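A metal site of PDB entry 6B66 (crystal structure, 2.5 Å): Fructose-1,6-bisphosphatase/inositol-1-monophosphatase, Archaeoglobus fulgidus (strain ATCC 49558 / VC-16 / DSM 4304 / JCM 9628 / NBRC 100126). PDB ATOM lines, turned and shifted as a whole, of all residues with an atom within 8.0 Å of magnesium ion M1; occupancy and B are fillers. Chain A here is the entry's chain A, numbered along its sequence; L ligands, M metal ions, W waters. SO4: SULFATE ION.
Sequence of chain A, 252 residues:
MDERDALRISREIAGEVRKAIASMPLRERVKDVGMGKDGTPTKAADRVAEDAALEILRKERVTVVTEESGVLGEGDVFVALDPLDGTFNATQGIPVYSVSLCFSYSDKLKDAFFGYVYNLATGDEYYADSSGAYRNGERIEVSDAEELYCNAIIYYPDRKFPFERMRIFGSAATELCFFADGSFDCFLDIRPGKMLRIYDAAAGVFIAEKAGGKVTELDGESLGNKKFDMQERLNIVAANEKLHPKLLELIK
The side-chain hydroxyl of Thr 40 sits close to the side-chain carboxylate of Glu 67.
The backbone NH (N) of Glu 67 sits at hydrogen-bond distance from the backbone carbonyl oxygen (O) of Leu 81 (3.5 Å).
The side-chain hydroxyl (OG1) of Thr 87 sits close to the backbone carbonyl oxygen (O) of Leu 84 (3.2 Å).
OE1 of Glu 67 is in salt-bridge range of NH1 of Arg 197 (3.3 Å).
The backbone NH (N) of Asp 38 sits at hydrogen-bond distance from the backbone carbonyl oxygen (O) of Glu 67 (3.3 Å).
Three residues have an atom within 4 Å of magnesium ion M1: Glu 67, Asp 82 and Leu 84.
Water W1 is bound to magnesium ion M1 (2.1 Å).
OE2 of Glu 67 binds magnesium ion M1.
The side-chain carboxylate (OD1) of Asp 82 is bound to magnesium ion M1 (2.1 Å).
The backbone carbonyl oxygen (O) of Leu 84 binds magnesium ion M1 (2.2 Å).
An oxygen (O2) of the ligand binds magnesium ion M1 (2.3 Å).
Magnesium ion M1 is bound by O3 of the ligand.
Water W1 lies within hydrogen-bond range of OE2 of Glu 68, OD1 of Asp 46 and N of Leu 84.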
ATOM      1  N   ASP A  38     -29.736  -0.141  10.359  1.00  0.00           N
ATOM      2  CA  ASP A  38     -30.704   0.884  10.765  1.00  0.00           C
ATOM      3  C   ASP A  38     -31.666   1.221   9.647  1.00  0.00           C
ATOM      4  O   ASP A  38     -32.668   1.910   9.870  1.00  0.00           O
ATOM      5  CB  ASP A  38     -29.987   2.157  11.204  1.00  0.00           C
ATOM      6  CG  ASP A  38     -29.430   2.943  10.034  1.00  0.00           C
ATOM      7  OD1 ASP A  38     -28.582   2.400   9.290  1.00  0.00           O
ATOM      8  OD2 ASP A  38     -29.842   4.096   9.829  1.00  0.00           O
ATOM      9  N   THR A  40     -30.486   2.869   6.766  1.00  0.00           N
ATOM     10  CA  THR A  40     -29.916   3.947   5.953  1.00  0.00           C
ATOM     11  C   THR A  40     -28.558   3.525   5.414  1.00  0.00           C
ATOM     12  O   THR A  40     -27.881   2.679   6.025  1.00  0.00           O
ATOM     13  CB  THR A  40     -29.758   5.262   6.741  1.00  0.00           C
ATOM     14  OG1 THR A  40     -28.796   5.075   7.796  1.00  0.00           O
ATOM     15  CG2 THR A  40     -31.114   5.727   7.297  1.00  0.00           C
ATOM     16  N   PRO A  41     -28.143   4.104   4.272  1.00  0.00           N
ATOM     17  CA  PRO A  41     -26.849   3.741   3.675  1.00  0.00           C
ATOM     18  C   PRO A  41     -25.690   3.816   4.677  1.00  0.00           C
ATOM     19  O   PRO A  41     -25.696   4.691   5.541  1.00  0.00           O
ATOM     20  CB  PRO A  41     -26.666   4.814   2.584  1.00  0.00           C
ATOM     21  CG  PRO A  41     -28.047   5.180   2.204  1.00  0.00           C
ATOM     22  CD  PRO A  41     -28.849   5.122   3.471  1.00  0.00           C
ATOM     23  N   ASP A  46     -18.530   5.651   7.698  1.00  0.00           N
ATOM     24  CA  ASP A  46     -19.260   4.909   8.742  1.00  0.00           C
ATOM     25  C   ASP A  46     -18.617   3.556   9.005  1.00  0.00           C
ATOM     26  O   ASP A  46     -18.373   3.189  10.165  1.00  0.00           O
ATOM     27  CB  ASP A  46     -20.735   4.697   8.375  1.00  0.00           C
ATOM     28  CG  ASP A  46     -21.522   6.000   8.307  1.00  0.00           C
ATOM     29  OD1 ASP A  46     -21.409   6.817   9.265  1.00  0.00           O
ATOM     30  OD2 ASP A  46     -22.247   6.201   7.301  1.00  0.00           O
ATOM     31  N   ALA A  49     -15.242   3.703  10.830  1.00  0.00           N
ATOM     32  CA  ALA A  49     -15.474   4.103  12.210  1.00  0.00           C
ATOM     33  C   ALA A  49     -15.963   2.918  13.005  1.00  0.00           C
ATOM     34  O   ALA A  49     -15.371   2.553  14.035  1.00  0.00           O
ATOM     35  CB  ALA A  49     -16.474   5.257  12.303  1.00  0.00           C
ATOM     36  N   GLU A  50     -17.023   2.289  12.523  1.00  0.00           N
ATOM     37  CA  GLU A  50     -17.622   1.188  13.257  1.00  0.00           C
ATOM     38  C   GLU A  50     -16.659   0.026  13.419  1.00  0.00           C
ATOM     39  O   GLU A  50     -16.586  -0.564  14.503  1.00  0.00           O
ATOM     40  CB  GLU A  50     -18.926   0.722  12.633  1.00  0.00           C
ATOM     41  CG  GLU A  50     -19.677  -0.266  13.516  1.00  0.00           C
ATOM     42  CD  GLU A  50     -21.033  -0.656  12.946  1.00  0.00           C
ATOM     43  OE1 GLU A  50     -22.068  -0.157  13.444  1.00  0.00           O
ATOM     44  OE2 GLU A  50     -21.083  -1.472  12.003  1.00  0.00           O
ATOM     45  N   THR A  66     -25.551  -0.710  17.544  1.00  0.00           N
ATOM     46  CA  THR A  66     -24.827   0.272  16.756  1.00  0.00           C
ATOM     47  C   THR A  66     -25.469   0.439  15.386  1.00  0.00           C
ATOM     48  O   THR A  66     -26.100  -0.476  14.862  1.00  0.00           O
ATOM     49  CB  THR A  66     -23.351  -0.155  16.612  1.00  0.00           C
ATOM     50  OG1 THR A  66     -22.679   0.754  15.729  1.00  0.00           O
ATOM     51  CG2 THR A  66     -23.268  -1.579  16.053  1.00  0.00           C
ATOM     52  N   GLU A  67     -25.296   1.611  14.791  1.00  0.00           N
ATOM     53  CA  GLU A  67     -26.081   1.995  13.630  1.00  0.00           C
ATOM     54  C   GLU A  67     -25.909   1.105  12.404  1.00  0.00           C
ATOM     55  O   GLU A  67     -26.884   0.706  11.776  1.00  0.00           O
ATOM     56  CB  GLU A  67     -25.820   3.441  13.224  1.00  0.00           C
ATOM     57  CG  GLU A  67     -26.649   3.859  12.037  1.00  0.00           C
ATOM     58  CD  GLU A  67     -26.258   5.204  11.497  1.00  0.00           C
ATOM     59  OE1 GLU A  67     -26.693   5.547  10.361  1.00  0.00           O
ATOM     60  OE2 GLU A  67     -25.503   5.905  12.224  1.00  0.00           O
ATOM     61  N   GLU A  68     -24.663   0.796  12.050  1.00  0.00           N
ATOM     62  CA  GLU A  68     -24.422   0.058  10.798  1.00  0.00           C
ATOM     63  C   GLU A  68     -24.677  -1.445  10.959  1.00  0.00           C
ATOM     64  O   GLU A  68     -25.384  -2.045  10.148  1.00  0.00           O
ATOM     65  CB  GLU A  68     -23.020   0.338  10.221  1.00  0.00           C
ATOM     66  CG  GLU A  68     -22.582   1.804  10.248  1.00  0.00           C
ATOM     67  CD  GLU A  68     -23.614   2.744   9.637  1.00  0.00           C
ATOM     68  OE1 GLU A  68     -24.347   2.320   8.709  1.00  0.00           O
ATOM     69  OE2 GLU A  68     -23.699   3.915  10.072  1.00  0.00           O
ATOM     70  N   LEU A  81     -24.039   2.673  20.443  1.00  0.00           N
ATOM     71  CA  LEU A  81     -22.899   3.204  19.680  1.00  0.00           C
ATOM     72  C   LEU A  81     -23.321   3.882  18.386  1.00  0.00           C
ATOM     73  O   LEU A  81     -23.951   3.264  17.513  1.00  0.00           O
ATOM     74  CB  LEU A  81     -21.901   2.077  19.365  1.00  0.00           C
ATOM     75  CG  LEU A  81     -20.773   2.391  18.369  1.00  0.00           C
ATOM     76  CD1 LEU A  81     -19.843   3.519  18.856  1.00  0.00           C
ATOM     77  CD2 LEU A  81     -19.967   1.133  18.093  1.00  0.00           C
ATOM     78  N   ASP A  82     -23.001   5.155  18.268  1.00  0.00           N
ATOM     79  CA  ASP A  82     -23.022   5.802  16.956  1.00  0.00           C
ATOM     80  C   ASP A  82     -21.554   5.967  16.595  1.00  0.00           C
ATOM     81  O   ASP A  82     -20.871   6.836  17.129  1.00  0.00           O
ATOM     82  CB  ASP A  82     -23.749   7.149  17.006  1.00  0.00           C
ATOM     83  CG  ASP A  82     -24.206   7.627  15.619  1.00  0.00           C
ATOM     84  OD1 ASP A  82     -23.723   7.071  14.591  1.00  0.00           O
ATOM     85  OD2 ASP A  82     -25.038   8.555  15.561  1.00  0.00           O
ATOM     86  N   PRO A  83     -21.057   5.101  15.709  1.00  0.00           N
ATOM     87  CA  PRO A  83     -19.624   5.102  15.401  1.00  0.00           C
ATOM     88  C   PRO A  83     -19.226   6.398  14.698  1.00  0.00           C
ATOM     89  O   PRO A  83     -18.088   6.859  14.820  1.00  0.00           O
ATOM     90  CB  PRO A  83     -19.462   3.898  14.475  1.00  0.00           C
ATOM     91  CG  PRO A  83     -20.794   3.720  13.844  1.00  0.00           C
ATOM     92  CD  PRO A  83     -21.814   4.160  14.853  1.00  0.00           C
ATOM     93  N   LEU A  84     -20.168   6.991  13.982  1.00  0.00           N
ATOM     94  CA  LEU A  84     -19.938   8.278  13.341  1.00  0.00           C
ATOM     95  C   LEU A  84     -21.266   9.023  13.260  1.00  0.00           C
ATOM     96  O   LEU A  84     -22.133   8.662  12.468  1.00  0.00           O
ATOM     97  CB  LEU A  84     -19.344   8.091  11.940  1.00  0.00           C
ATOM     98  CG  LEU A  84     -19.073   9.368  11.136  1.00  0.00           C
ATOM     99  CD1 LEU A  84     -18.163  10.313  11.919  1.00  0.00           C
ATOM    100  CD2 LEU A  84     -18.492   9.056   9.746  1.00  0.00           C
ATOM    101  N   ASP A  85     -21.416  10.051  14.089  1.00  0.00           N
ATOM    102  CA  ASP A  85     -22.641  10.830  14.133  1.00  0.00           C
ATOM    103  C   ASP A  85     -22.320  12.157  13.486  1.00  0.00           C
ATOM    104  O   ASP A  85     -21.371  12.812  13.885  1.00  0.00           O
ATOM    105  CB  ASP A  85     -23.103  11.030  15.573  1.00  0.00           C
ATOM    106  CG  ASP A  85     -24.415  11.790  15.658  1.00  0.00           C
ATOM    107  OD1 ASP A  85     -25.430  11.274  15.131  1.00  0.00           O
ATOM    108  OD2 ASP A  85     -24.434  12.898  16.248  1.00  0.00           O
ATOM    109  N   GLY A  86     -23.107  12.528  12.479  1.00  0.00           N
ATOM    110  CA  GLY A  86     -22.761  13.673  11.654  1.00  0.00           C
ATOM    111  C   GLY A  86     -22.011  13.277  10.382  1.00  0.00           C
ATOM    112  O   GLY A  86     -21.203  14.041   9.858  1.00  0.00           O
ATOM    113  N   THR A  87     -22.289  12.066   9.886  1.00  0.00           N
ATOM    114  CA  THR A  87     -21.584  11.530   8.712  1.00  0.00           C
ATOM    115  C   THR A  87     -21.517  12.518   7.524  1.00  0.00           C
ATOM    116  O   THR A  87     -20.480  12.627   6.856  1.00  0.00           O
ATOM    117  CB  THR A  87     -22.187  10.185   8.244  1.00  0.00           C
ATOM    118  OG1 THR A  87     -22.187   9.233   9.331  1.00  0.00           O
ATOM    119  CG2 THR A  87     -21.374   9.607   7.084  1.00  0.00           C
ATOM    120  N   SER A  98     -18.850  13.211  15.333  1.00  0.00           N
ATOM    121  CA  SER A  98     -18.417  12.607  16.581  1.00  0.00           C
ATOM    122  C   SER A  98     -18.635  11.114  16.593  1.00  0.00           C
ATOM    123  O   SER A  98     -19.367  10.576  15.769  1.00  0.00           O
ATOM    124  CB  SER A  98     -19.224  13.196  17.749  1.00  0.00           C
ATOM    125  OG  SER A  98     -18.939  14.578  17.920  1.00  0.00           O
ATOM    126  N   VAL A  99     -17.993  10.446  17.543  1.00  0.00           N
ATOM    127  CA  VAL A  99     -18.387   9.100  17.913  1.00  0.00           C
ATOM    128  C   VAL A  99     -19.067   9.221  19.287  1.00  0.00           C
ATOM    129  O   VAL A  99     -18.640  10.011  20.145  1.00  0.00           O
ATOM    130  CB  VAL A  99     -17.191   8.152  17.968  1.00  0.00           C
ATOM    131  CG1 VAL A  99     -16.126   8.688  18.908  1.00  0.00           C
ATOM    132  CG2 VAL A  99     -17.643   6.765  18.400  1.00  0.00           C
ATOM    133  N   ARG A 197     -32.521   7.960  16.713  1.00  0.00           N
ATOM    134  CA  ARG A 197     -32.425   6.596  17.218  1.00  0.00           C
ATOM    135  C   ARG A 197     -31.650   6.600  18.540  1.00  0.00           C
ATOM    136  O   ARG A 197     -31.007   7.596  18.888  1.00  0.00           O
ATOM    137  CB  ARG A 197     -31.795   5.714  16.158  1.00  0.00           C
ATOM    138  CG  ARG A 197     -32.626   5.676  14.874  1.00  0.00           C
ATOM    139  CD  ARG A 197     -31.779   5.584  13.622  1.00  0.00           C
ATOM    140  NE  ARG A 197     -30.900   6.739  13.447  1.00  0.00           N
ATOM    141  CZ  ARG A 197     -29.813   6.721  12.690  1.00  0.00           C
ATOM    142  NH1 ARG A 197     -29.485   5.606  12.056  1.00  0.00           N
ATOM    143  NH2 ARG A 197     -29.061   7.813  12.568  1.00  0.00           N
ATOM    144  N   TYR A 199     -28.931   5.522  19.585  1.00  0.00           N
ATOM    145  CA  TYR A 199     -27.485   5.759  19.579  1.00  0.00           C
ATOM    146  C   TYR A 199     -27.139   7.188  19.197  1.00  0.00           C
ATOM    147  O   TYR A 199     -26.035   7.660  19.503  1.00  0.00           O
ATOM    148  CB  TYR A 199     -26.736   4.744  18.703  1.00  0.00           C
ATOM    149  CG  TYR A 199     -27.469   4.410  17.436  1.00  0.00           C
ATOM    150  CD1 TYR A 199     -28.146   3.197  17.309  1.00  0.00           C
ATOM    151  CD2 TYR A 199     -27.515   5.299  16.367  1.00  0.00           C
ATOM    152  CE1 TYR A 199     -28.838   2.882  16.156  1.00  0.00           C
ATOM    153  CE2 TYR A 199     -28.200   4.991  15.212  1.00  0.00           C
ATOM    154  CZ  TYR A 199     -28.865   3.776  15.119  1.00  0.00           C
ATOM    155  OH  TYR A 199     -29.563   3.444  13.982  1.00  0.00           O
ATOM    156  N   ASP A 200     -28.073   7.878  18.564  1.00  0.00           N
ATOM    157  CA  ASP A 200     -27.928   9.323  18.318  1.00  0.00           C
ATOM    158  C   ASP A 200     -28.007  10.142  19.609  1.00  0.00           C
ATOM    159  O   ASP A 200     -27.244  11.084  19.806  1.00  0.00           O
ATOM    160  CB  ASP A 200     -29.041   9.809  17.390  1.00  0.00           C
ATOM    161  CG  ASP A 200     -28.910   9.257  15.978  1.00  0.00           C
ATOM    162  OD1 ASP A 200     -27.785   9.303  15.436  1.00  0.00           O
ATOM    163  OD2 ASP A 200     -29.949   8.777  15.447  1.00  0.00           O
HETATM  164  S   SO4 L   1     -25.645   9.353  11.487  1.00  0.00           S
HETATM  165  O1  SO4 L   1     -27.009   9.113  10.981  1.00  0.00           O
HETATM  166  O2  SO4 L   1     -24.702   8.473  10.752  1.00  0.00           O
HETATM  167  O3  SO4 L   1     -25.605   9.089  12.943  1.00  0.00           O
HETATM  168  O4  SO4 L   1     -25.286  10.767  11.250  1.00  0.00           O
HETATM  169 MG    MG M   1     -23.863   7.265  12.460  1.00  0.00          MG
HETATM  170 MG    MG M   2     -26.989   3.707   8.212  1.00  0.00          MG
HETATM  171  O   HOH W   1     -22.505   5.857  11.723  1.00  0.00           O
